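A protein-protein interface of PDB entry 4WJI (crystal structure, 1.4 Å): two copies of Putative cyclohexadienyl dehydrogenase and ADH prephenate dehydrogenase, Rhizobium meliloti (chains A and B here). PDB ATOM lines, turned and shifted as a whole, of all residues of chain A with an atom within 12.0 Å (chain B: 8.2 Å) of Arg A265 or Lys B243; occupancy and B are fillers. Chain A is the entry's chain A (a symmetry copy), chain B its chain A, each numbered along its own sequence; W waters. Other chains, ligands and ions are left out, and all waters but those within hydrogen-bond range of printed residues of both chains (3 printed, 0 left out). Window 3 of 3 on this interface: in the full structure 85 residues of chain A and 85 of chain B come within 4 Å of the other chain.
The backbone carbonyl oxygen of Arg A265 lies within hydrogen-bond range of the side-chain amino group of Lys B243, 3.2 Å away.
The side-chain amide oxygen (OE1) of Gln A261 sits at hydrogen-bond distance from the guanidinium group (NE) of Arg A265 (2.8 Å).
Among the printed residues, pairs that only touch across the chains: Leu A257 with Leu B250, Leu A260 with Ile B193, Gln A261 with Leu B247, Ile A264 with Ile B193, Ile A264 with Cys B239, Ile A264 with Lys B243, Ile A264 with Leu B247, Ile A264 with Leu B250, Arg A265 with Leu B247, Gly A267 with Leu B240 and Leu A272 with Cys B239.
Printed residues of chain B within 4 Å of Gln A261: Leu B247 (3.9 Å). Of the printed residues of chain B, Ile A264 touches Ile B193, Cys B239, Lys B243, Leu B247 and Leu B250. Of chain B, only Lys B243 and Leu B247 come within 4 Å of Arg A265. Printed residues of chain B within 4 Å of Gly A267: Leu B240. Lys A271 touches none of the printed residues of chain B. Ala B185 touches none of the printed residues of chain A. Cys B239 touches just these residues of chain A: Ile A264 (3.9 Å) and Leu A272 (3.8 Å). Printed residues of chain A within 4 Å of Leu B240: Gly A267. No residue of chain A comes within 4 Å of Asn B242. Of the printed residues of chain A, Lys B243 touches Ile A264 (3.9 Å) and Arg A265 (3.2 Å). No residue of chain A comes within 4 Å of Asp B244. No residue of chain A comes within 4 Å of Ile B246. Leu B247 touches three residues of chain A. The nearest printed residue of chain B that does not touch Gln A261 is Leu B250 (4.1 Å).
Of the 20 printed residues of chain B, 6 touch a printed residue of chain A. Printed residues of chain B that touch a printed residue of chain A: Ile B193, Cys B239, Leu B240, Lys B243, Leu B247 and Leu B250. Hydrophobic or aromatic side chains of chain B within 4 Å of the printed part of chain A: Ile B193, Leu B240, Leu B247 and Leu B250. Printed residues of chain A that touch a printed residue of chain B: Leu A257, Leu A260, Gln A261, Ile A264, Arg A265, Gly A267 and Leu A272. Hydrophobic or aromatic side chains of chain A that line the printed part of chain B: Leu A257, Leu A260, Ile A264 and Leu A272. Among the printed residues, 12 pairs touch across the chains. Among the printed residues, no Asp or Glu carboxylate lies within 4 Å of a Lys or Arg side-chain nitrogen of the other chain.
No position is printed for both chains. Of the 12 pairs that touch across the chains among the printed residues, none has its exchanged pair printed and touching as well.
Water W2 lies within hydrogen-bond range of the backbone carbonyl oxygen (O) of Arg A265 (2.6 Å) and the side-chain amino group (NZ) of Lys B243 (2.9 Å). Water W3 lies within hydrogen-bond range of O of Leu B247 (2.8 Å) and NE2 of Gln A261 (3.0 Å). Water W1 bridges the backbone carbonyl oxygen of Ile A264 and the backbone carbonyl oxygen of Cys B239.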
ATOM      1  N   SER A 254       7.896 -19.951  13.517  1.00  0.00           N
ATOM      2  CA  SER A 254       8.339 -18.939  14.431  1.00  0.00           C
ATOM      3  C   SER A 254       9.396 -19.390  15.424  1.00  0.00           C
ATOM      4  O   SER A 254      10.321 -18.597  15.714  1.00  0.00           O
ATOM      5  CB  SER A 254       7.168 -18.293  15.141  1.00  0.00           C
ATOM      6  OG  SER A 254       6.368 -17.582  14.208  1.00  0.00           O
ATOM      7  N   GLU A 255       9.349 -20.647  15.836  1.00  0.00           N
ATOM      8  CA  GLU A 255      10.427 -21.245  16.685  1.00  0.00           C
ATOM      9  C   GLU A 255      11.740 -21.218  15.901  1.00  0.00           C
ATOM     10  O   GLU A 255      12.778 -20.801  16.408  1.00  0.00           O
ATOM     11  CB  GLU A 255      10.128 -22.701  17.081  1.00  0.00           C
ATOM     12  N   ASP A 256      11.672 -21.630  14.633  1.00  0.00           N
ATOM     13  CA  ASP A 256      12.862 -21.696  13.775  1.00  0.00           C
ATOM     14  C   ASP A 256      13.400 -20.308  13.483  1.00  0.00           C
ATOM     15  O   ASP A 256      14.645 -20.093  13.511  1.00  0.00           O
ATOM     16  CB  ASP A 256      12.507 -22.402  12.475  1.00  0.00           C
ATOM     17  CG  ASP A 256      12.349 -23.933  12.635  1.00  0.00           C
ATOM     18  OD1 ASP A 256      12.565 -24.505  13.749  1.00  0.00           O
ATOM     19  OD2 ASP A 256      11.976 -24.600  11.635  1.00  0.00           O
ATOM     20  N   LEU A 257      12.510 -19.323  13.277  1.00  0.00           N
ATOM     21  CA  LEU A 257      12.970 -17.976  13.010  1.00  0.00           C
ATOM     22  C   LEU A 257      13.657 -17.362  14.223  1.00  0.00           C
ATOM     23  O   LEU A 257      14.628 -16.644  14.075  1.00  0.00           O
ATOM     24  CB  LEU A 257      11.813 -17.090  12.533  1.00  0.00           C
ATOM     25  CG  LEU A 257      12.224 -15.745  11.954  1.00  0.00           C
ATOM     26  CD1 LEU A 257      13.122 -15.905  10.721  1.00  0.00           C
ATOM     27  CD2 LEU A 257      11.019 -14.880  11.594  1.00  0.00           C
ATOM     28  N   ALA A 258      13.166 -17.630  15.432  1.00  0.00           N
ATOM     29  CA  ALA A 258      13.887 -17.169  16.654  1.00  0.00           C
ATOM     30  C   ALA A 258      15.293 -17.668  16.719  1.00  0.00           C
ATOM     31  O   ALA A 258      16.213 -16.930  17.109  1.00  0.00           O
ATOM     32  CB  ALA A 258      13.139 -17.623  17.914  1.00  0.00           C
ATOM     33  N   SER A 259      15.495 -18.913  16.338  1.00  0.00           N
ATOM     34  CA  SER A 259      16.839 -19.507  16.326  1.00  0.00           C
ATOM     35  C   SER A 259      17.730 -18.887  15.240  1.00  0.00           C
ATOM     36  O   SER A 259      18.913 -18.591  15.471  1.00  0.00           O
ATOM     37  CB  SER A 259      16.733 -21.012  16.125  1.00  0.00           C
ATOM     38  OG  SER A 259      16.036 -21.610  17.199  1.00  0.00           O
ATOM     39  N   LEU A 260      17.178 -18.651  14.066  1.00  0.00           N
ATOM     40  CA  LEU A 260      17.929 -17.963  13.013  1.00  0.00           C
ATOM     41  C   LEU A 260      18.275 -16.515  13.413  1.00  0.00           C
ATOM     42  O   LEU A 260      19.393 -16.063  13.205  1.00  0.00           O
ATOM     43  CB  LEU A 260      17.122 -18.002  11.708  1.00  0.00           C
ATOM     44  CG  LEU A 260      17.769 -17.612  10.396  1.00  0.00           C
ATOM     45  CD1 LEU A 260      19.107 -18.271  10.212  1.00  0.00           C
ATOM     46  CD2 LEU A 260      16.810 -18.017   9.270  1.00  0.00           C
ATOM     47  N   GLN A 261      17.324 -15.798  14.021  1.00  0.00           N
ATOM     48  CA  GLN A 261      17.546 -14.472  14.509  1.00  0.00           C
ATOM     49  C   GLN A 261      18.703 -14.471  15.535  1.00  0.00           C
ATOM     50  O   GLN A 261      19.553 -13.543  15.515  1.00  0.00           O
ATOM     51  CB  GLN A 261      16.266 -13.925  15.123  1.00  0.00           C
ATOM     52  CG  GLN A 261      16.267 -12.470  15.487  1.00  0.00           C
ATOM     53  CD  GLN A 261      16.733 -12.234  16.905  1.00  0.00           C
ATOM     54  OE1 GLN A 261      17.134 -13.174  17.617  1.00  0.00           O
ATOM     55  NE2 GLN A 261      16.698 -10.973  17.330  1.00  0.00           N
ATOM     56  N   ARG A 262      18.749 -15.475  16.398  1.00  0.00           N
ATOM     57  CA  ARG A 262      19.817 -15.560  17.397  1.00  0.00           C
ATOM     58  C   ARG A 262      21.176 -15.820  16.725  1.00  0.00           C
ATOM     59  O   ARG A 262      22.183 -15.193  17.105  1.00  0.00           O
ATOM     60  CB  ARG A 262      19.500 -16.667  18.392  1.00  0.00           C
ATOM     61  CG  ARG A 262      20.432 -16.674  19.571  1.00  0.00           C
ATOM     62  CD  ARG A 262      19.990 -17.631  20.688  1.00  0.00           C
ATOM     63  NE  ARG A 262      20.078 -19.014  20.212  1.00  0.00           N
ATOM     64  CZ  ARG A 262      19.045 -19.815  19.949  1.00  0.00           C
ATOM     65  NH1 ARG A 262      17.790 -19.413  20.155  1.00  0.00           N
ATOM     66  NH2 ARG A 262      19.270 -21.048  19.493  1.00  0.00           N
ATOM     67  N   ALA A 263      21.225 -16.701  15.722  1.00  0.00           N
ATOM     68  CA  ALA A 263      22.472 -16.905  14.937  1.00  0.00           C
ATOM     69  C   ALA A 263      22.954 -15.605  14.272  1.00  0.00           C
ATOM     70  O   ALA A 263      24.162 -15.306  14.263  1.00  0.00           O
ATOM     71  CB  ALA A 263      22.278 -17.981  13.889  1.00  0.00           C
ATOM     72  N   ILE A 264      22.031 -14.787  13.759  1.00  0.00           N
ATOM     73  CA  ILE A 264      22.429 -13.501  13.195  1.00  0.00           C
ATOM     74  C   ILE A 264      22.923 -12.525  14.299  1.00  0.00           C
ATOM     75  O   ILE A 264      23.972 -11.879  14.173  1.00  0.00           O
ATOM     76  CB  ILE A 264      21.275 -12.878  12.377  1.00  0.00           C
ATOM     77  CG1 ILE A 264      20.933 -13.760  11.168  1.00  0.00           C
ATOM     78  CG2 ILE A 264      21.652 -11.503  11.868  1.00  0.00           C
ATOM     79  CD1 ILE A 264      19.697 -13.312  10.402  1.00  0.00           C
ATOM     80  N   ARG A 265      22.184 -12.447  15.402  1.00  0.00           N
ATOM     81  CA  ARG A 265      22.587 -11.645  16.540  1.00  0.00           C
ATOM     82  C   ARG A 265      23.979 -11.975  17.060  1.00  0.00           C
ATOM     83  O   ARG A 265      24.723 -11.045  17.462  1.00  0.00           O
ATOM     84  CB  ARG A 265      21.590 -11.824  17.731  1.00  0.00           C
ATOM     85  CG  ARG A 265      20.449 -10.840  17.818  1.00  0.00           C
ATOM     86  CD  ARG A 265      19.706 -10.837  19.187  1.00  0.00           C
ATOM     87  NE  ARG A 265      18.968 -12.089  19.446  1.00  0.00           N
ATOM     88  CZ  ARG A 265      19.156 -12.910  20.495  1.00  0.00           C
ATOM     89  NH1 ARG A 265      20.076 -12.653  21.417  1.00  0.00           N
ATOM     90  NH2 ARG A 265      18.440 -14.018  20.612  1.00  0.00           N
ATOM     91  N   TRP A 266      24.333 -13.273  17.068  1.00  0.00           N
ATOM     92  CA  TRP A 266      25.603 -13.721  17.653  1.00  0.00           C
ATOM     93  C   TRP A 266      26.681 -13.945  16.622  1.00  0.00           C
ATOM     94  O   TRP A 266      27.782 -14.430  16.947  1.00  0.00           O
ATOM     95  CB  TRP A 266      25.347 -15.007  18.435  1.00  0.00           C
ATOM     96  CG  TRP A 266      24.540 -14.799  19.701  1.00  0.00           C
ATOM     97  CD1 TRP A 266      24.218 -13.615  20.277  1.00  0.00           C
ATOM     98  CD2 TRP A 266      24.079 -15.814  20.590  1.00  0.00           C
ATOM     99  NE1 TRP A 266      23.528 -13.824  21.457  1.00  0.00           N
ATOM    100  CE2 TRP A 266      23.433 -15.171  21.668  1.00  0.00           C
ATOM    101  CE3 TRP A 266      24.113 -17.208  20.561  1.00  0.00           C
ATOM    102  CZ2 TRP A 266      22.834 -15.880  22.720  1.00  0.00           C
ATOM    103  CZ3 TRP A 266      23.516 -17.909  21.610  1.00  0.00           C
ATOM    104  CH2 TRP A 266      22.898 -17.241  22.677  1.00  0.00           C
ATOM    105  N   GLY A 267      26.386 -13.604  15.363  1.00  0.00           N
ATOM    106  CA  GLY A 267      27.371 -13.777  14.321  1.00  0.00           C
ATOM    107  C   GLY A 267      27.840 -15.216  14.114  1.00  0.00           C
ATOM    108  O   GLY A 267      29.020 -15.462  13.818  1.00  0.00           O
ATOM    109  N   ASP A 268      26.912 -16.177  14.210  1.00  0.00           N
ATOM    110  CA  ASP A 268      27.274 -17.568  14.076  1.00  0.00           C
ATOM    111  C   ASP A 268      27.253 -17.981  12.599  1.00  0.00           C
ATOM    112  O   ASP A 268      26.284 -18.596  12.087  1.00  0.00           O
ATOM    113  CB  ASP A 268      26.362 -18.467  14.925  1.00  0.00           C
ATOM    114  CG  ASP A 268      26.878 -19.904  14.994  1.00  0.00           C
ATOM    115  OD1 ASP A 268      27.824 -20.273  14.236  1.00  0.00           O
ATOM    116  OD2 ASP A 268      26.315 -20.663  15.804  1.00  0.00           O
ATOM    117  N   GLY A 269      28.339 -17.637  11.918  1.00  0.00           N
ATOM    118  CA  GLY A 269      28.437 -17.855  10.481  1.00  0.00           C
ATOM    119  C   GLY A 269      28.339 -19.321  10.125  1.00  0.00           C
ATOM    120  O   GLY A 269      27.801 -19.634   9.060  1.00  0.00           O
ATOM    121  N   ASP A 270      28.886 -20.212  10.967  1.00  0.00           N
ATOM    122  CA  ASP A 270      28.874 -21.625  10.644  1.00  0.00           C
ATOM    123  C   ASP A 270      27.438 -22.186  10.672  1.00  0.00           C
ATOM    124  O   ASP A 270      27.048 -22.951   9.780  1.00  0.00           O
ATOM    125  CB  ASP A 270      29.801 -22.414  11.581  1.00  0.00           C
ATOM    126  N   LYS A 271      26.641 -21.774  11.656  1.00  0.00           N
ATOM    127  CA  LYS A 271      25.222 -22.172  11.738  1.00  0.00           C
ATOM    128  C   LYS A 271      24.431 -21.677  10.510  1.00  0.00           C
ATOM    129  O   LYS A 271      23.635 -22.412   9.901  1.00  0.00           O
ATOM    130  CB  LYS A 271      24.570 -21.625  13.021  1.00  0.00           C
ATOM    131  CG  LYS A 271      23.175 -22.131  13.320  1.00  0.00           C
ATOM    132  N   LEU A 272      24.677 -20.422  10.130  1.00  0.00           N
ATOM    133  CA  LEU A 272      24.018 -19.848   8.964  1.00  0.00           C
ATOM    134  C   LEU A 272      24.386 -20.605   7.708  1.00  0.00           C
ATOM    135  O   LEU A 272      23.516 -20.976   6.926  1.00  0.00           O
ATOM    136  CB  LEU A 272      24.403 -18.381   8.805  1.00  0.00           C
ATOM    137  CG  LEU A 272      23.912 -17.469   9.948  1.00  0.00           C
ATOM    138  CD1 LEU A 272      24.486 -16.069   9.812  1.00  0.00           C
ATOM    139  CD2 LEU A 272      22.387 -17.426  10.001  1.00  0.00           C
ATOM    140  N   PHE A 276      21.763 -22.703   5.261  1.00  0.00           N
ATOM    141  CA  PHE A 276      21.626 -22.297   3.867  1.00  0.00           C
ATOM    142  C   PHE A 276      22.076 -23.392   2.894  1.00  0.00           C
ATOM    143  O   PHE A 276      21.575 -23.482   1.769  1.00  0.00           O
ATOM    144  CB  PHE A 276      22.412 -20.993   3.615  1.00  0.00           C
ATOM    145  CG  PHE A 276      21.981 -19.822   4.470  1.00  0.00           C
ATOM    146  CD1 PHE A 276      20.784 -19.818   5.195  1.00  0.00           C
ATOM    147  CD2 PHE A 276      22.805 -18.694   4.558  1.00  0.00           C
ATOM    148  CE1 PHE A 276      20.426 -18.735   5.961  1.00  0.00           C
ATOM    149  CE2 PHE A 276      22.440 -17.605   5.307  1.00  0.00           C
ATOM    150  CZ  PHE A 276      21.262 -17.616   6.026  1.00  0.00           C
ATOM    151  N   THR B 100      25.800  -5.741   0.352  1.00  0.00           N
ATOM    152  CA  THR B 100      25.909  -4.796   1.457  1.00  0.00           C
ATOM    153  C   THR B 100      26.903  -3.699   1.051  1.00  0.00           C
ATOM    154  O   THR B 100      27.770  -3.931   0.210  1.00  0.00           O
ATOM    155  CB  THR B 100      26.350  -5.468   2.790  1.00  0.00           C
ATOM    156  OG1 THR B 100      27.711  -5.843   2.702  1.00  0.00           O
ATOM    157  CG2 THR B 100      25.560  -6.697   3.065  1.00  0.00           C
ATOM    158  N   SER B 103      29.556  -2.136   5.207  1.00  0.00           N
ATOM    159  CA  SER B 103      30.639  -3.035   5.557  1.00  0.00           C
ATOM    160  C   SER B 103      31.755  -3.023   4.542  1.00  0.00           C
ATOM    161  O   SER B 103      32.941  -3.022   4.902  1.00  0.00           O
ATOM    162  CB  SER B 103      30.182  -4.482   5.772  1.00  0.00           C
ATOM    163  OG  SER B 103      29.765  -5.091   4.542  1.00  0.00           O
ATOM    164  N   ASP B 181      21.747   0.120   3.067  1.00  0.00           N
ATOM    165  CA  ASP B 181      21.701  -1.062   3.870  1.00  0.00           C
ATOM    166  C   ASP B 181      20.321  -1.270   4.545  1.00  0.00           C
ATOM    167  O   ASP B 181      19.865  -2.414   4.667  1.00  0.00           O
ATOM    168  CB  ASP B 181      22.872  -1.098   4.865  1.00  0.00           C
ATOM    169  CG  ASP B 181      24.260  -1.334   4.166  1.00  0.00           C
ATOM    170  OD1 ASP B 181      24.312  -1.662   2.944  1.00  0.00           O
ATOM    171  OD2 ASP B 181      25.309  -1.190   4.871  1.00  0.00           O
ATOM    172  N   ALA B 185      17.852  -4.313   3.366  1.00  0.00           N
ATOM    173  CA  ALA B 185      17.428  -5.207   4.432  1.00  0.00           C
ATOM    174  C   ALA B 185      15.982  -5.636   4.234  1.00  0.00           C
ATOM    175  O   ALA B 185      15.681  -6.782   4.466  1.00  0.00           O
ATOM    176  CB  ALA B 185      17.635  -4.591   5.815  1.00  0.00           C
ATOM    177  N   HIS B 189      17.260  -8.727   1.834  1.00  0.00           N
ATOM    178  CA  HIS B 189      17.834  -9.593   2.824  1.00  0.00           C
ATOM    179  C   HIS B 189      16.796 -10.341   3.657  1.00  0.00           C
ATOM    180  O   HIS B 189      16.893 -11.558   3.786  1.00  0.00           O
ATOM    181  CB  HIS B 189      18.866  -8.855   3.693  1.00  0.00           C
ATOM    182  CG  HIS B 189      19.901  -8.151   2.869  1.00  0.00           C
ATOM    183  ND1 HIS B 189      20.677  -7.134   3.384  1.00  0.00           N
ATOM    184  CD2 HIS B 189      20.219  -8.245   1.555  1.00  0.00           C
ATOM    185  CE1 HIS B 189      21.481  -6.683   2.439  1.00  0.00           C
ATOM    186  NE2 HIS B 189      21.208  -7.337   1.307  1.00  0.00           N
ATOM    187  N   ILE B 193      16.149 -14.429   3.990  1.00  0.00           N
ATOM    188  CA  ILE B 193      16.174 -15.052   5.308  1.00  0.00           C
ATOM    189  C   ILE B 193      14.869 -15.817   5.603  1.00  0.00           C
ATOM    190  O   ILE B 193      14.933 -16.955   6.061  1.00  0.00           O
ATOM    191  CB  ILE B 193      16.434 -14.002   6.387  1.00  0.00           C
ATOM    192  CG1 ILE B 193      17.895 -13.544   6.282  1.00  0.00           C
ATOM    193  CG2 ILE B 193      16.092 -14.509   7.790  1.00  0.00           C
ATOM    194  CD1 ILE B 193      18.178 -12.215   6.989  1.00  0.00           C
ATOM    195  N   ASP B 237      27.552 -14.310   4.328  1.00  0.00           N
ATOM    196  CA  ASP B 237      28.251 -13.035   4.446  1.00  0.00           C
ATOM    197  C   ASP B 237      27.302 -11.829   4.569  1.00  0.00           C
ATOM    198  O   ASP B 237      27.577 -10.892   5.323  1.00  0.00           O
ATOM    199  CB  ASP B 237      29.237 -12.857   3.308  1.00  0.00           C
ATOM    200  CG  ASP B 237      30.486 -13.699   3.471  1.00  0.00           C
ATOM    201  OD1 ASP B 237      30.609 -14.537   4.423  1.00  0.00           O
ATOM    202  OD2 ASP B 237      31.427 -13.451   2.636  1.00  0.00           O
ATOM    203  N   VAL B 238      26.201 -11.807   3.799  1.00  0.00           N
ATOM    204  CA  VAL B 238      25.245 -10.702   3.952  1.00  0.00           C
ATOM    205  C   VAL B 238      24.702 -10.614   5.384  1.00  0.00           C
ATOM    206  O   VAL B 238      24.588  -9.517   5.957  1.00  0.00           O
ATOM    207  CB  VAL B 238      24.073 -10.860   2.941  1.00  0.00           C
ATOM    208  CG1 VAL B 238      22.977  -9.870   3.225  1.00  0.00           C
ATOM    209  CG2 VAL B 238      24.545 -10.631   1.539  1.00  0.00           C
ATOM    210  N   CYS B 239      24.333 -11.755   5.967  1.00  0.00           N
ATOM    211  CA  CYS B 239      23.800 -11.762   7.327  1.00  0.00           C
ATOM    212  C   CYS B 239      24.831 -11.285   8.355  1.00  0.00           C
ATOM    213  O   CYS B 239      24.470 -10.633   9.353  1.00  0.00           O
ATOM    214  CB  CYS B 239      23.352 -13.175   7.714  1.00  0.00           C
ATOM    215  SG  CYS B 239      21.852 -13.709   6.870  1.00  0.00           S
ATOM    216  N   LEU B 240      26.081 -11.624   8.118  1.00  0.00           N
ATOM    217  CA  LEU B 240      27.183 -11.199   9.025  1.00  0.00           C
ATOM    218  C   LEU B 240      27.501  -9.709   8.887  1.00  0.00           C
ATOM    219  O   LEU B 240      27.957  -9.075   9.838  1.00  0.00           O
ATOM    220  CB  LEU B 240      28.466 -11.993   8.747  1.00  0.00           C
ATOM    221  CG  LEU B 240      28.416 -13.496   9.108  1.00  0.00           C
ATOM    222  CD1 LEU B 240      29.624 -14.254   8.572  1.00  0.00           C
ATOM    223  CD2 LEU B 240      28.248 -13.709  10.600  1.00  0.00           C
ATOM    224  N   HIS B 241      27.319  -9.164   7.698  1.00  0.00           N
ATOM    225  CA  HIS B 241      27.739  -7.803   7.381  1.00  0.00           C
ATOM    226  C   HIS B 241      26.644  -6.760   7.238  1.00  0.00           C
ATOM    227  O   HIS B 241      26.954  -5.577   7.088  1.00  0.00           O
ATOM    228  CB  HIS B 241      28.664  -7.862   6.141  1.00  0.00           C
ATOM    229  CG  HIS B 241      29.961  -8.480   6.486  1.00  0.00           C
ATOM    230  ND1 HIS B 241      30.319  -9.772   6.217  1.00  0.00           N
ATOM    231  CD2 HIS B 241      30.957  -7.959   7.245  1.00  0.00           C
ATOM    232  CE1 HIS B 241      31.519 -10.004   6.747  1.00  0.00           C
ATOM    233  NE2 HIS B 241      31.914  -8.924   7.377  1.00  0.00           N
ATOM    234  N   ASN B 242      25.388  -7.165   7.330  1.00  0.00           N
ATOM    235  CA  ASN B 242      24.293  -6.178   7.446  1.00  0.00           C
ATOM    236  C   ASN B 242      23.450  -6.450   8.689  1.00  0.00           C
ATOM    237  O   ASN B 242      22.227  -6.282   8.668  1.00  0.00           O
ATOM    238  CB  ASN B 242      23.397  -6.168   6.193  1.00  0.00           C
ATOM    239  CG  ASN B 242      22.587  -4.883   6.077  1.00  0.00           C
ATOM    240  OD1 ASN B 242      22.978  -3.852   6.609  1.00  0.00           O
ATOM    241  ND2 ASN B 242      21.504  -4.922   5.316  1.00  0.00           N
ATOM    242  N   LYS B 243      24.117  -6.877   9.764  1.00  0.00           N
ATOM    243  CA  LYS B 243      23.447  -7.369  10.958  1.00  0.00           C
ATOM    244  C   LYS B 243      22.407  -6.403  11.517  1.00  0.00           C
ATOM    245  O   LYS B 243      21.268  -6.816  11.782  1.00  0.00           O
ATOM    246  CB  LYS B 243      24.535  -7.674  12.028  1.00  0.00           C
ATOM    247  CG  LYS B 243      23.995  -8.049  13.396  1.00  0.00           C
ATOM    248  CD  LYS B 243      25.160  -8.006  14.399  1.00  0.00           C
ATOM    249  CE  LYS B 243      24.732  -8.347  15.759  1.00  0.00           C
ATOM    250  NZ  LYS B 243      25.872  -8.213  16.687  1.00  0.00           N
ATOM    251  N   ASP B 244      22.771  -5.158  11.779  1.00  0.00           N
ATOM    252  CA  ASP B 244      21.888  -4.282  12.515  1.00  0.00           C
ATOM    253  C   ASP B 244      20.584  -3.988  11.731  1.00  0.00           C
ATOM    254  O   ASP B 244      19.487  -4.073  12.296  1.00  0.00           O
ATOM    255  CB  ASP B 244      22.614  -3.002  12.917  1.00  0.00           C
ATOM    256  CG  ASP B 244      23.507  -3.173  14.174  1.00  0.00           C
ATOM    257  OD1 ASP B 244      23.656  -4.289  14.758  1.00  0.00           O
ATOM    258  OD2 ASP B 244      24.067  -2.146  14.589  1.00  0.00           O
ATOM    259  N   ALA B 245      20.714  -3.724  10.436  1.00  0.00           N
ATOM    260  CA  ALA B 245      19.522  -3.439   9.625  1.00  0.00           C
ATOM    261  C   ALA B 245      18.644  -4.671   9.455  1.00  0.00           C
ATOM    262  O   ALA B 245      17.414  -4.569   9.531  1.00  0.00           O
ATOM    263  CB  ALA B 245      19.897  -2.885   8.272  1.00  0.00           C
ATOM    264  N   ILE B 246      19.277  -5.826   9.277  1.00  0.00           N
ATOM    265  CA  ILE B 246      18.539  -7.060   9.201  1.00  0.00           C
ATOM    266  C   ILE B 246      17.756  -7.325  10.491  1.00  0.00           C
ATOM    267  O   ILE B 246      16.583  -7.740  10.457  1.00  0.00           O
ATOM    268  CB  ILE B 246      19.485  -8.235   8.833  1.00  0.00           C
ATOM    269  CG1 ILE B 246      19.892  -8.106   7.351  1.00  0.00           C
ATOM    270  CG2 ILE B 246      18.845  -9.573   9.124  1.00  0.00           C
ATOM    271  CD1 ILE B 246      20.972  -9.059   6.913  1.00  0.00           C
ATOM    272  N   LEU B 247      18.412  -7.181  11.643  1.00  0.00           N
ATOM    273  CA  LEU B 247      17.744  -7.459  12.916  1.00  0.00           C
ATOM    274  C   LEU B 247      16.570  -6.509  13.110  1.00  0.00           C
ATOM    275  O   LEU B 247      15.530  -6.935  13.639  1.00  0.00           O
ATOM    276  CB  LEU B 247      18.729  -7.360  14.095  1.00  0.00           C
ATOM    277  CG  LEU B 247      19.727  -8.500  14.152  1.00  0.00           C
ATOM    278  CD1 LEU B 247      20.812  -8.292  15.239  1.00  0.00           C
ATOM    279  CD2 LEU B 247      19.079  -9.850  14.355  1.00  0.00           C
ATOM    280  N   GLU B 248      16.703  -5.250  12.696  1.00  0.00           N
ATOM    281  CA  GLU B 248      15.580  -4.298  12.802  1.00  0.00           C
ATOM    282  C   GLU B 248      14.389  -4.794  11.954  1.00  0.00           C
ATOM    283  O   GLU B 248      13.229  -4.817  12.444  1.00  0.00           O
ATOM    284  CB  GLU B 248      15.954  -2.881  12.389  1.00  0.00           C
ATOM    285  CG  GLU B 248      14.818  -1.854  12.429  1.00  0.00           C
ATOM    286  N   MET B 249      14.643  -5.226  10.729  1.00  0.00           N
ATOM    287  CA  MET B 249      13.554  -5.681   9.865  1.00  0.00           C
ATOM    288  C   MET B 249      12.966  -6.994  10.362  1.00  0.00           C
ATOM    289  O   MET B 249      11.721  -7.172  10.278  1.00  0.00           O
ATOM    290  CB  MET B 249      14.050  -5.798   8.422  1.00  0.00           C
ATOM    291  CG  MET B 249      14.472  -4.437   7.840  1.00  0.00           C
ATOM    292  SD  MET B 249      13.014  -3.109   7.910  1.00  0.00           S
ATOM    293  CE  MET B 249      14.096  -1.705   7.037  1.00  0.00           C
ATOM    294  N   LEU B 250      13.805  -7.916  10.877  1.00  0.00           N
ATOM    295  CA  LEU B 250      13.285  -9.150  11.469  1.00  0.00           C
ATOM    296  C   LEU B 250      12.353  -8.839  12.642  1.00  0.00           C
ATOM    297  O   LEU B 250      11.308  -9.502  12.779  1.00  0.00           O
ATOM    298  CB  LEU B 250      14.375 -10.107  11.934  1.00  0.00           C
ATOM    299  CG  LEU B 250      15.034 -10.959  10.887  1.00  0.00           C
ATOM    300  CD1 LEU B 250      16.293 -11.584  11.438  1.00  0.00           C
ATOM    301  CD2 LEU B 250      14.103 -12.070  10.429  1.00  0.00           C
HETATM  302  O   HOH W   1      25.586 -11.266  11.995  1.00  0.00           O
HETATM  303  O   HOH W   2      23.810  -8.920  18.542  1.00  0.00           O
HETATM  304  O   HOH W   3      15.475  -8.786  15.682  1.00  0.00           O
